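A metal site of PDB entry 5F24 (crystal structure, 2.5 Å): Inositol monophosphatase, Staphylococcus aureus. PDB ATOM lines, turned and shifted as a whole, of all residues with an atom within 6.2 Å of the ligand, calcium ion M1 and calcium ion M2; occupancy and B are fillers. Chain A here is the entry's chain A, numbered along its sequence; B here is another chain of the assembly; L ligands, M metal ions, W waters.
The backbone NH of Gly 92 lies within hydrogen-bond range of an oxygen (O7) of the ligand (2.6 Å). The backbone NH (N) of Thr 93 is in hydrogen-bond range of an oxygen (O7) of the ligand, 2.8 Å away. The side-chain amide nitrogen (ND2) of Asn 202 is in hydrogen-bond range of an oxygen (O5) of the ligand, at 2.9 Å. An oxygen (O2) of the ligand is in hydrogen-bond range of the backbone NH of Cys 185, 3.0 Å away. The backbone carbonyl oxygen (O) of Gly 183 sits at hydrogen-bond distance from an oxygen (O3) of the ligand (2.9 Å).
OD2 of Asp 47 touches calcium ion M1 (3.8 Å). OG1 of Thr 93 touches calcium ion M1 (3.9 Å). Of the 25 residues printed, 5 come within 4 Å of calcium ion M1. The nearest printed residue that does not touch calcium ion M1 is Glu 71 (4.2 Å).
The nearest printed residue that does not touch calcium ion M2 is Glu 70 (4.3 Å).
Calcium ion M2 is bound by O1 of the ligand (2.3 Å), OD1 of Asp 209 (2.3 Å), OD2 of Asp 88 (2.3 Å), OD1 of Asp 91 (2.3 Å), water W2 (2.3 Å) and O8 of the ligand (2.4 Å). Calcium ion M2 has six donor atoms within binding distance.
Water W6 lies within hydrogen-bond range of OG1 of Thr 93 (2.6 Å) and O9 of the ligand (2.8 Å). Water W2 bridges the indole nitrogen of Trp 208 (3.3 Å) and the side-chain carboxylate of Glu 70 (3.4 Å). Water W7 lies within hydrogen-bond range of an oxygen (O6) of the ligand and the side-chain carboxylate (OD2) of Asp 209. Water W3 lies within hydrogen-bond range of O7 of the ligand (2.6 Å), N of Ala 94 (3.1 Å) and N of Thr 93 (3.2 Å). Water W4 bridges an oxygen (O3) of the ligand and the side-chain carboxylate (OD2) of Asp 188. Water W1 lies within hydrogen-bond range of a ring nitrogen (NE2) of His 200 (2.7 Å), the side-chain amide nitrogen (ND2) of Asn 202 (2.9 Å), an oxygen (O4) of the ligand (3.2 Å) and the side-chain sulfur (SG) of Cys 185 (3.6 Å).
The side-chain carboxylate of Asp 91 lies within hydrogen-bond range of the backbone NH of Gly 186, at 2.8 Å. The side-chain carboxylate of Asp 188 is in hydrogen-bond range of the backbone NH of Gly 183 (2.8 Å). The backbone carbonyl oxygen (O) of Asp 209 lies within hydrogen-bond range of the side-chain sulfur (SG) of Cys 185 (3.3 Å). N of Asp 88 is in hydrogen-bond range of O of Ile 106, 2.9 Å away. NE1 of Trp 208 sits close to OE2 of Glu 70, at 3.5 Å. N of Cys 185 is in hydrogen-bond range of OD2 of Asp 91. The side-chain carboxylate (OD2) of Asp 188 lies within hydrogen-bond range of the backbone NH (N) of Ala 184, 3.2 Å away. The side-chain amide oxygen (OD1) of Asn 202 sits at hydrogen-bond distance from the backbone NH (N) of Asn 204 (2.8 Å).
Calcium ion M1 is bound by water W8 (2.3 Å), the side-chain carboxylate (OE2) of Glu 70 (2.3 Å), an oxygen (O8) of the ligand (2.3 Å), the backbone carbonyl oxygen (O) of Ile 90 (2.3 Å), water W6 (2.3 Å) and the side-chain carboxylate (OD1) of Asp 88 (2.3 Å).
Residues that only touch the ligand: Ala 184 (3.5 Å).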
ATOM      1  N   ASP A  47     -13.039 -14.755  -6.683  1.00  0.00           N
ATOM      2  CA  ASP A  47     -13.537 -15.896  -7.455  1.00  0.00           C
ATOM      3  C   ASP A  47     -13.737 -15.496  -8.909  1.00  0.00           C
ATOM      4  O   ASP A  47     -13.251 -16.184  -9.809  1.00  0.00           O
ATOM      5  CB  ASP A  47     -14.856 -16.423  -6.879  1.00  0.00           C
ATOM      6  CG  ASP A  47     -14.770 -16.781  -5.396  1.00  0.00           C
ATOM      7  OD1 ASP A  47     -14.395 -15.907  -4.568  1.00  0.00           O
ATOM      8  OD2 ASP A  47     -15.154 -17.913  -5.028  1.00  0.00           O
ATOM      9  N   GLU A  70     -17.619 -23.012 -11.397  1.00  0.00           N
ATOM     10  CA  GLU A  70     -18.658 -22.616 -10.421  1.00  0.00           C
ATOM     11  C   GLU A  70     -19.390 -21.369 -10.852  1.00  0.00           C
ATOM     12  O   GLU A  70     -20.612 -21.292 -10.811  1.00  0.00           O
ATOM     13  CB  GLU A  70     -18.072 -22.418  -9.016  1.00  0.00           C
ATOM     14  CG  GLU A  70     -19.153 -22.030  -7.978  1.00  0.00           C
ATOM     15  CD  GLU A  70     -18.694 -22.254  -6.549  1.00  0.00           C
ATOM     16  OE1 GLU A  70     -19.535 -22.123  -5.653  1.00  0.00           O
ATOM     17  OE2 GLU A  70     -17.498 -22.565  -6.358  1.00  0.00           O
ATOM     18  N   GLU A  71     -18.641 -20.341 -11.243  1.00  0.00           N
ATOM     19  CA  GLU A  71     -19.207 -18.984 -11.419  1.00  0.00           C
ATOM     20  C   GLU A  71     -19.770 -18.737 -12.843  1.00  0.00           C
ATOM     21  O   GLU A  71     -19.889 -17.628 -13.291  1.00  0.00           O
ATOM     22  CB  GLU A  71     -18.165 -17.880 -11.086  1.00  0.00           C
ATOM     23  CG  GLU A  71     -17.390 -18.054  -9.769  1.00  0.00           C
ATOM     24  CD  GLU A  71     -18.277 -18.227  -8.535  1.00  0.00           C
ATOM     25  OE1 GLU A  71     -19.392 -17.638  -8.492  1.00  0.00           O
ATOM     26  OE2 GLU A  71     -17.851 -18.962  -7.628  1.00  0.00           O
ATOM     27  N   ASP A  88     -12.694 -24.828  -9.826  1.00  0.00           N
ATOM     28  CA  ASP A  88     -13.201 -24.030  -8.715  1.00  0.00           C
ATOM     29  C   ASP A  88     -12.226 -22.880  -8.480  1.00  0.00           C
ATOM     30  O   ASP A  88     -11.068 -23.071  -8.033  1.00  0.00           O
ATOM     31  CB  ASP A  88     -13.419 -24.802  -7.437  1.00  0.00           C
ATOM     32  CG  ASP A  88     -14.278 -24.049  -6.451  1.00  0.00           C
ATOM     33  OD1 ASP A  88     -14.315 -22.802  -6.547  1.00  0.00           O
ATOM     34  OD2 ASP A  88     -14.910 -24.712  -5.579  1.00  0.00           O
ATOM     35  N   PRO A  89     -12.623 -21.679  -8.865  1.00  0.00           N
ATOM     36  CA  PRO A  89     -11.606 -20.599  -8.879  1.00  0.00           C
ATOM     37  C   PRO A  89     -11.145 -20.230  -7.483  1.00  0.00           C
ATOM     38  O   PRO A  89      -9.973 -19.893  -7.321  1.00  0.00           O
ATOM     39  CB  PRO A  89     -12.326 -19.439  -9.570  1.00  0.00           C
ATOM     40  CG  PRO A  89     -13.781 -19.737  -9.413  1.00  0.00           C
ATOM     41  CD  PRO A  89     -13.899 -21.220  -9.427  1.00  0.00           C
ATOM     42  N   ILE A  90     -12.030 -20.243  -6.507  1.00  0.00           N
ATOM     43  CA  ILE A  90     -11.627 -20.274  -5.094  1.00  0.00           C
ATOM     44  C   ILE A  90     -12.447 -21.358  -4.391  1.00  0.00           C
ATOM     45  O   ILE A  90     -13.656 -21.260  -4.301  1.00  0.00           O
ATOM     46  CB  ILE A  90     -11.893 -18.937  -4.401  1.00  0.00           C
ATOM     47  CG1 ILE A  90     -11.023 -17.850  -5.010  1.00  0.00           C
ATOM     48  CG2 ILE A  90     -11.612 -19.065  -2.913  1.00  0.00           C
ATOM     49  CD1 ILE A  90      -9.534 -17.994  -4.727  1.00  0.00           C
ATOM     50  N   ASP A  91     -11.768 -22.379  -3.912  1.00  0.00           N
ATOM     51  CA  ASP A  91     -12.429 -23.373  -3.046  1.00  0.00           C
ATOM     52  C   ASP A  91     -12.075 -22.966  -1.658  1.00  0.00           C
ATOM     53  O   ASP A  91     -10.931 -22.788  -1.377  1.00  0.00           O
ATOM     54  CB  ASP A  91     -11.988 -24.796  -3.356  1.00  0.00           C
ATOM     55  CG  ASP A  91     -12.672 -25.850  -2.489  1.00  0.00           C
ATOM     56  OD1 ASP A  91     -13.919 -25.843  -2.383  1.00  0.00           O
ATOM     57  OD2 ASP A  91     -11.936 -26.655  -1.883  1.00  0.00           O
ATOM     58  N   GLY A  92     -13.039 -22.842  -0.784  1.00  0.00           N
ATOM     59  CA  GLY A  92     -12.824 -22.259   0.560  1.00  0.00           C
ATOM     60  C   GLY A  92     -13.063 -20.766   0.657  1.00  0.00           C
ATOM     61  O   GLY A  92     -12.305 -20.023   1.311  1.00  0.00           O
ATOM     62  N   THR A  93     -14.082 -20.292  -0.040  1.00  0.00           N
ATOM     63  CA  THR A  93     -14.404 -18.845  -0.106  1.00  0.00           C
ATOM     64  C   THR A  93     -14.641 -18.313   1.310  1.00  0.00           C
ATOM     65  O   THR A  93     -14.240 -17.200   1.630  1.00  0.00           O
ATOM     66  CB  THR A  93     -15.632 -18.621  -1.050  1.00  0.00           C
ATOM     67  OG1 THR A  93     -15.256 -18.925  -2.418  1.00  0.00           O
ATOM     68  CG2 THR A  93     -16.112 -17.226  -1.042  1.00  0.00           C
ATOM     69  N   ALA A  94     -15.279 -19.097   2.172  1.00  0.00           N
ATOM     70  CA  ALA A  94     -15.526 -18.678   3.542  1.00  0.00           C
ATOM     71  C   ALA A  94     -14.207 -18.403   4.241  1.00  0.00           C
ATOM     72  O   ALA A  94     -14.048 -17.354   4.864  1.00  0.00           O
ATOM     73  CB  ALA A  94     -16.325 -19.726   4.294  1.00  0.00           C
ATOM     74  N   ILE A 106      -8.767 -24.894  -7.653  1.00  0.00           N
ATOM     75  CA  ILE A 106      -8.862 -26.261  -8.157  1.00  0.00           C
ATOM     76  C   ILE A 106      -9.069 -26.279  -9.700  1.00  0.00           C
ATOM     77  O   ILE A 106      -9.968 -25.640 -10.222  1.00  0.00           O
ATOM     78  CB  ILE A 106     -10.020 -26.995  -7.455  1.00  0.00           C
ATOM     79  CG1 ILE A 106      -9.855 -26.981  -5.936  1.00  0.00           C
ATOM     80  CG2 ILE A 106     -10.085 -28.454  -7.887  1.00  0.00           C
ATOM     81  CD1 ILE A 106     -10.948 -27.695  -5.170  1.00  0.00           C
ATOM     82  N   ASN A 160     -17.681 -32.099   7.573  1.00  0.00           N
ATOM     83  CA  ASN A 160     -18.535 -31.043   8.126  1.00  0.00           C
ATOM     84  C   ASN A 160     -19.514 -31.680   9.095  1.00  0.00           C
ATOM     85  O   ASN A 160     -20.444 -32.383   8.675  1.00  0.00           O
ATOM     86  CB  ASN A 160     -19.305 -30.314   7.030  1.00  0.00           C
ATOM     87  CG  ASN A 160     -20.153 -29.164   7.564  1.00  0.00           C
ATOM     88  OD1 ASN A 160     -20.305 -29.011   8.760  1.00  0.00           O
ATOM     89  ND2 ASN A 160     -20.719 -28.361   6.660  1.00  0.00           N
ATOM     90  N   LEU A 181     -10.630 -29.984  10.884  1.00  0.00           N
ATOM     91  CA  LEU A 181     -11.230 -29.422   9.671  1.00  0.00           C
ATOM     92  C   LEU A 181     -10.418 -28.234   9.199  1.00  0.00           C
ATOM     93  O   LEU A 181     -10.321 -27.216   9.879  1.00  0.00           O
ATOM     94  CB  LEU A 181     -12.683 -29.025   9.918  1.00  0.00           C
ATOM     95  CG  LEU A 181     -13.478 -28.530   8.698  1.00  0.00           C
ATOM     96  CD1 LEU A 181     -13.537 -29.517   7.566  1.00  0.00           C
ATOM     97  CD2 LEU A 181     -14.895 -28.186   9.117  1.00  0.00           C
ATOM     98  N   GLY A 183     -11.379 -26.861   6.093  1.00  0.00           N
ATOM     99  CA  GLY A 183     -12.557 -26.109   5.656  1.00  0.00           C
ATOM    100  C   GLY A 183     -12.561 -25.763   4.171  1.00  0.00           C
ATOM    101  O   GLY A 183     -13.308 -24.895   3.724  1.00  0.00           O
ATOM    102  N   ALA A 184     -11.656 -26.349   3.426  1.00  0.00           N
ATOM    103  CA  ALA A 184     -11.734 -26.276   1.963  1.00  0.00           C
ATOM    104  C   ALA A 184     -11.618 -27.665   1.413  1.00  0.00           C
ATOM    105  O   ALA A 184     -10.610 -28.314   1.630  1.00  0.00           O
ATOM    106  CB  ALA A 184     -10.663 -25.387   1.390  1.00  0.00           C
ATOM    107  N   CYS A 185     -12.616 -28.127   0.659  1.00  0.00           N
ATOM    108  CA  CYS A 185     -12.637 -29.520   0.153  1.00  0.00           C
ATOM    109  C   CYS A 185     -11.315 -29.938  -0.485  1.00  0.00           C
ATOM    110  O   CYS A 185     -10.810 -31.022  -0.181  1.00  0.00           O
ATOM    111  CB  CYS A 185     -13.747 -29.700  -0.837  1.00  0.00           C
ATOM    112  SG  CYS A 185     -14.017 -31.424  -1.323  1.00  0.00           S
ATOM    113  N   GLY A 186     -10.787 -29.116  -1.369  1.00  0.00           N
ATOM    114  CA  GLY A 186      -9.494 -29.361  -1.978  1.00  0.00           C
ATOM    115  C   GLY A 186      -8.356 -29.562  -0.988  1.00  0.00           C
ATOM    116  O   GLY A 186      -7.476 -30.424  -1.175  1.00  0.00           O
ATOM    117  N   ASP A 188      -8.592 -30.193   2.510  1.00  0.00           N
ATOM    118  CA  ASP A 188      -8.874 -31.344   3.322  1.00  0.00           C
ATOM    119  C   ASP A 188      -8.615 -32.635   2.530  1.00  0.00           C
ATOM    120  O   ASP A 188      -8.088 -33.605   3.070  1.00  0.00           O
ATOM    121  CB  ASP A 188     -10.313 -31.327   3.813  1.00  0.00           C
ATOM    122  CG  ASP A 188     -10.561 -30.276   4.895  1.00  0.00           C
ATOM    123  OD1 ASP A 188     -10.181 -30.519   6.041  1.00  0.00           O
ATOM    124  OD2 ASP A 188     -11.189 -29.236   4.617  1.00  0.00           O
ATOM    125  N   HIS A 200     -11.516 -37.705   4.143  1.00  0.00           N
ATOM    126  CA  HIS A 200     -12.319 -36.512   4.117  1.00  0.00           C
ATOM    127  C   HIS A 200     -13.670 -36.858   3.513  1.00  0.00           C
ATOM    128  O   HIS A 200     -13.720 -37.578   2.502  1.00  0.00           O
ATOM    129  CB  HIS A 200     -11.623 -35.362   3.379  1.00  0.00           C
ATOM    130  CG  HIS A 200     -12.483 -34.149   3.226  1.00  0.00           C
ATOM    131  ND1 HIS A 200     -12.899 -33.388   4.290  1.00  0.00           N
ATOM    132  CD2 HIS A 200     -13.060 -33.589   2.125  1.00  0.00           C
ATOM    133  CE1 HIS A 200     -13.670 -32.395   3.864  1.00  0.00           C
ATOM    134  NE2 HIS A 200     -13.799 -32.514   2.551  1.00  0.00           N
ATOM    135  N   ASN A 202     -17.430 -35.220   2.090  1.00  0.00           N
ATOM    136  CA  ASN A 202     -18.316 -34.117   1.765  1.00  0.00           C
ATOM    137  C   ASN A 202     -19.657 -34.681   1.268  1.00  0.00           C
ATOM    138  O   ASN A 202     -19.737 -35.360   0.219  1.00  0.00           O
ATOM    139  CB  ASN A 202     -17.735 -33.231   0.685  1.00  0.00           C
ATOM    140  CG  ASN A 202     -18.581 -31.977   0.438  1.00  0.00           C
ATOM    141  OD1 ASN A 202     -19.798 -32.054   0.253  1.00  0.00           O
ATOM    142  ND2 ASN A 202     -17.938 -30.821   0.419  1.00  0.00           N
ATOM    143  N   ASN A 204     -22.314 -33.357   0.025  1.00  0.00           N
ATOM    144  CA  ASN A 204     -23.009 -32.775  -1.112  1.00  0.00           C
ATOM    145  C   ASN A 204     -22.091 -31.899  -1.989  1.00  0.00           C
ATOM    146  O   ASN A 204     -22.306 -30.688  -2.080  1.00  0.00           O
ATOM    147  CB  ASN A 204     -24.147 -31.909  -0.589  1.00  0.00           C
ATOM    148  CG  ASN A 204     -25.123 -31.470  -1.676  1.00  0.00           C
ATOM    149  OD1 ASN A 204     -25.947 -30.597  -1.431  1.00  0.00           O
ATOM    150  ND2 ASN A 204     -25.069 -32.093  -2.831  1.00  0.00           N
ATOM    151  N   PRO A 205     -21.055 -32.497  -2.571  1.00  0.00           N
ATOM    152  CA  PRO A 205     -20.143 -31.688  -3.399  1.00  0.00           C
ATOM    153  C   PRO A 205     -20.618 -31.402  -4.804  1.00  0.00           C
ATOM    154  O   PRO A 205     -21.332 -32.179  -5.371  1.00  0.00           O
ATOM    155  CB  PRO A 205     -18.924 -32.590  -3.491  1.00  0.00           C
ATOM    156  CG  PRO A 205     -19.512 -33.966  -3.512  1.00  0.00           C
ATOM    157  CD  PRO A 205     -20.682 -33.920  -2.567  1.00  0.00           C
ATOM    158  N   TRP A 208     -16.950 -29.355  -9.306  1.00  0.00           N
ATOM    159  CA  TRP A 208     -15.704 -28.561  -9.133  1.00  0.00           C
ATOM    160  C   TRP A 208     -15.034 -28.770  -7.798  1.00  0.00           C
ATOM    161  O   TRP A 208     -13.829 -28.598  -7.702  1.00  0.00           O
ATOM    162  CB  TRP A 208     -15.876 -27.093  -9.465  1.00  0.00           C
ATOM    163  CG  TRP A 208     -17.120 -26.524  -8.966  1.00  0.00           C
ATOM    164  CD1 TRP A 208     -17.351 -26.033  -7.731  1.00  0.00           C
ATOM    165  CD2 TRP A 208     -18.326 -26.363  -9.701  1.00  0.00           C
ATOM    166  NE1 TRP A 208     -18.633 -25.595  -7.631  1.00  0.00           N
ATOM    167  CE2 TRP A 208     -19.263 -25.801  -8.811  1.00  0.00           C
ATOM    168  CE3 TRP A 208     -18.724 -26.671 -11.003  1.00  0.00           C
ATOM    169  CZ2 TRP A 208     -20.580 -25.511  -9.202  1.00  0.00           C
ATOM    170  CZ3 TRP A 208     -20.051 -26.382 -11.393  1.00  0.00           C
ATOM    171  CH2 TRP A 208     -20.958 -25.804 -10.491  1.00  0.00           C
ATOM    172  N   ASP A 209     -15.778 -29.118  -6.756  1.00  0.00           N
ATOM    173  CA  ASP A 209     -15.200 -29.409  -5.427  1.00  0.00           C
ATOM    174  C   ASP A 209     -14.321 -30.636  -5.396  1.00  0.00           C
ATOM    175  O   ASP A 209     -13.401 -30.752  -4.543  1.00  0.00           O
ATOM    176  CB  ASP A 209     -16.323 -29.780  -4.448  1.00  0.00           C
ATOM    177  CG  ASP A 209     -17.144 -28.601  -4.009  1.00  0.00           C
ATOM    178  OD1 ASP A 209     -16.565 -27.544  -3.704  1.00  0.00           O
ATOM    179  OD2 ASP A 209     -18.390 -28.747  -3.979  1.00  0.00           O
ATOM    180  N   ARG B 180     -14.252 -24.399  12.701  1.00  0.00           N
ATOM    181  CA  ARG B 180     -12.985 -24.959  12.236  1.00  0.00           C
ATOM    182  C   ARG B 180     -12.190 -25.417  13.408  1.00  0.00           C
ATOM    183  O   ARG B 180     -12.439 -25.031  14.536  1.00  0.00           O
ATOM    184  CB  ARG B 180     -12.056 -24.035  11.423  1.00  0.00           C
ATOM    185  CG  ARG B 180     -12.613 -23.151  10.322  1.00  0.00           C
ATOM    186  CD  ARG B 180     -12.585 -23.717   8.908  1.00  0.00           C
ATOM    187  NE  ARG B 180     -13.966 -24.017   8.629  1.00  0.00           N
ATOM    188  CZ  ARG B 180     -14.753 -23.483   7.714  1.00  0.00           C
ATOM    189  NH1 ARG B 180     -14.354 -22.640   6.781  1.00  0.00           N
ATOM    190  NH2 ARG B 180     -15.989 -23.871   7.737  1.00  0.00           N
HETATM  191  C1  LIG L   1     -17.028 -25.132  -0.324  1.00  0.00           C
HETATM  192  C2  LIG L   1     -15.805 -25.634   0.442  1.00  0.00           C
HETATM  193  C3  LIG L   1     -16.233 -26.101   1.830  1.00  0.00           C
HETATM  194  C4  LIG L   1     -17.583 -26.856   1.962  1.00  0.00           C
HETATM  195  C5  LIG L   1     -18.545 -26.853   0.775  1.00  0.00           C
HETATM  196  C6  LIG L   1     -18.013 -26.256  -0.529  1.00  0.00           C
HETATM  197  P1  LIG L   1     -16.557 -22.972  -1.856  1.00  0.00           P
HETATM  198  O1  LIG L   1     -16.679 -24.587  -1.595  1.00  0.00           O
HETATM  199  O2  LIG L   1     -15.050 -26.617  -0.276  1.00  0.00           O
HETATM  200  O3  LIG L   1     -15.197 -26.747   2.577  1.00  0.00           O
HETATM  201  O4  LIG L   1     -17.455 -28.162   2.537  1.00  0.00           O
HETATM  202  O5  LIG L   1     -19.011 -28.170   0.549  1.00  0.00           O
HETATM  203  O6  LIG L   1     -19.174 -25.737  -1.173  1.00  0.00           O
HETATM  204  O7  LIG L   1     -15.613 -22.530  -0.783  1.00  0.00           O
HETATM  205  O8  LIG L   1     -16.068 -23.031  -3.287  1.00  0.00           O
HETATM  206  O9  LIG L   1     -17.942 -22.409  -1.626  1.00  0.00           O
HETATM  207 CA    CA M   1     -15.773 -21.670  -5.126  1.00  0.00          CA
HETATM  208 CA    CA M   2     -15.866 -25.360  -3.588  1.00  0.00          CA
HETATM  209  O   HOH W   1     -15.456 -30.520   1.854  1.00  0.00           O
HETATM  210  O   HOH W   2     -17.958 -24.858  -4.511  1.00  0.00           O
HETATM  211  O   HOH W   3     -16.094 -22.008   1.721  1.00  0.00           O
HETATM  212  O   HOH W   4     -13.987 -29.008   3.780  1.00  0.00           O
HETATM  213  O   HOH W   5     -16.378 -28.832   5.017  1.00  0.00           O
HETATM  214  O   HOH W   6     -17.007 -20.548  -3.518  1.00  0.00           O
HETATM  215  O   HOH W   7     -19.804 -26.565  -3.346  1.00  0.00           O
HETATM  216  O   HOH W   8     -15.590 -19.765  -6.340  1.00  0.00           O
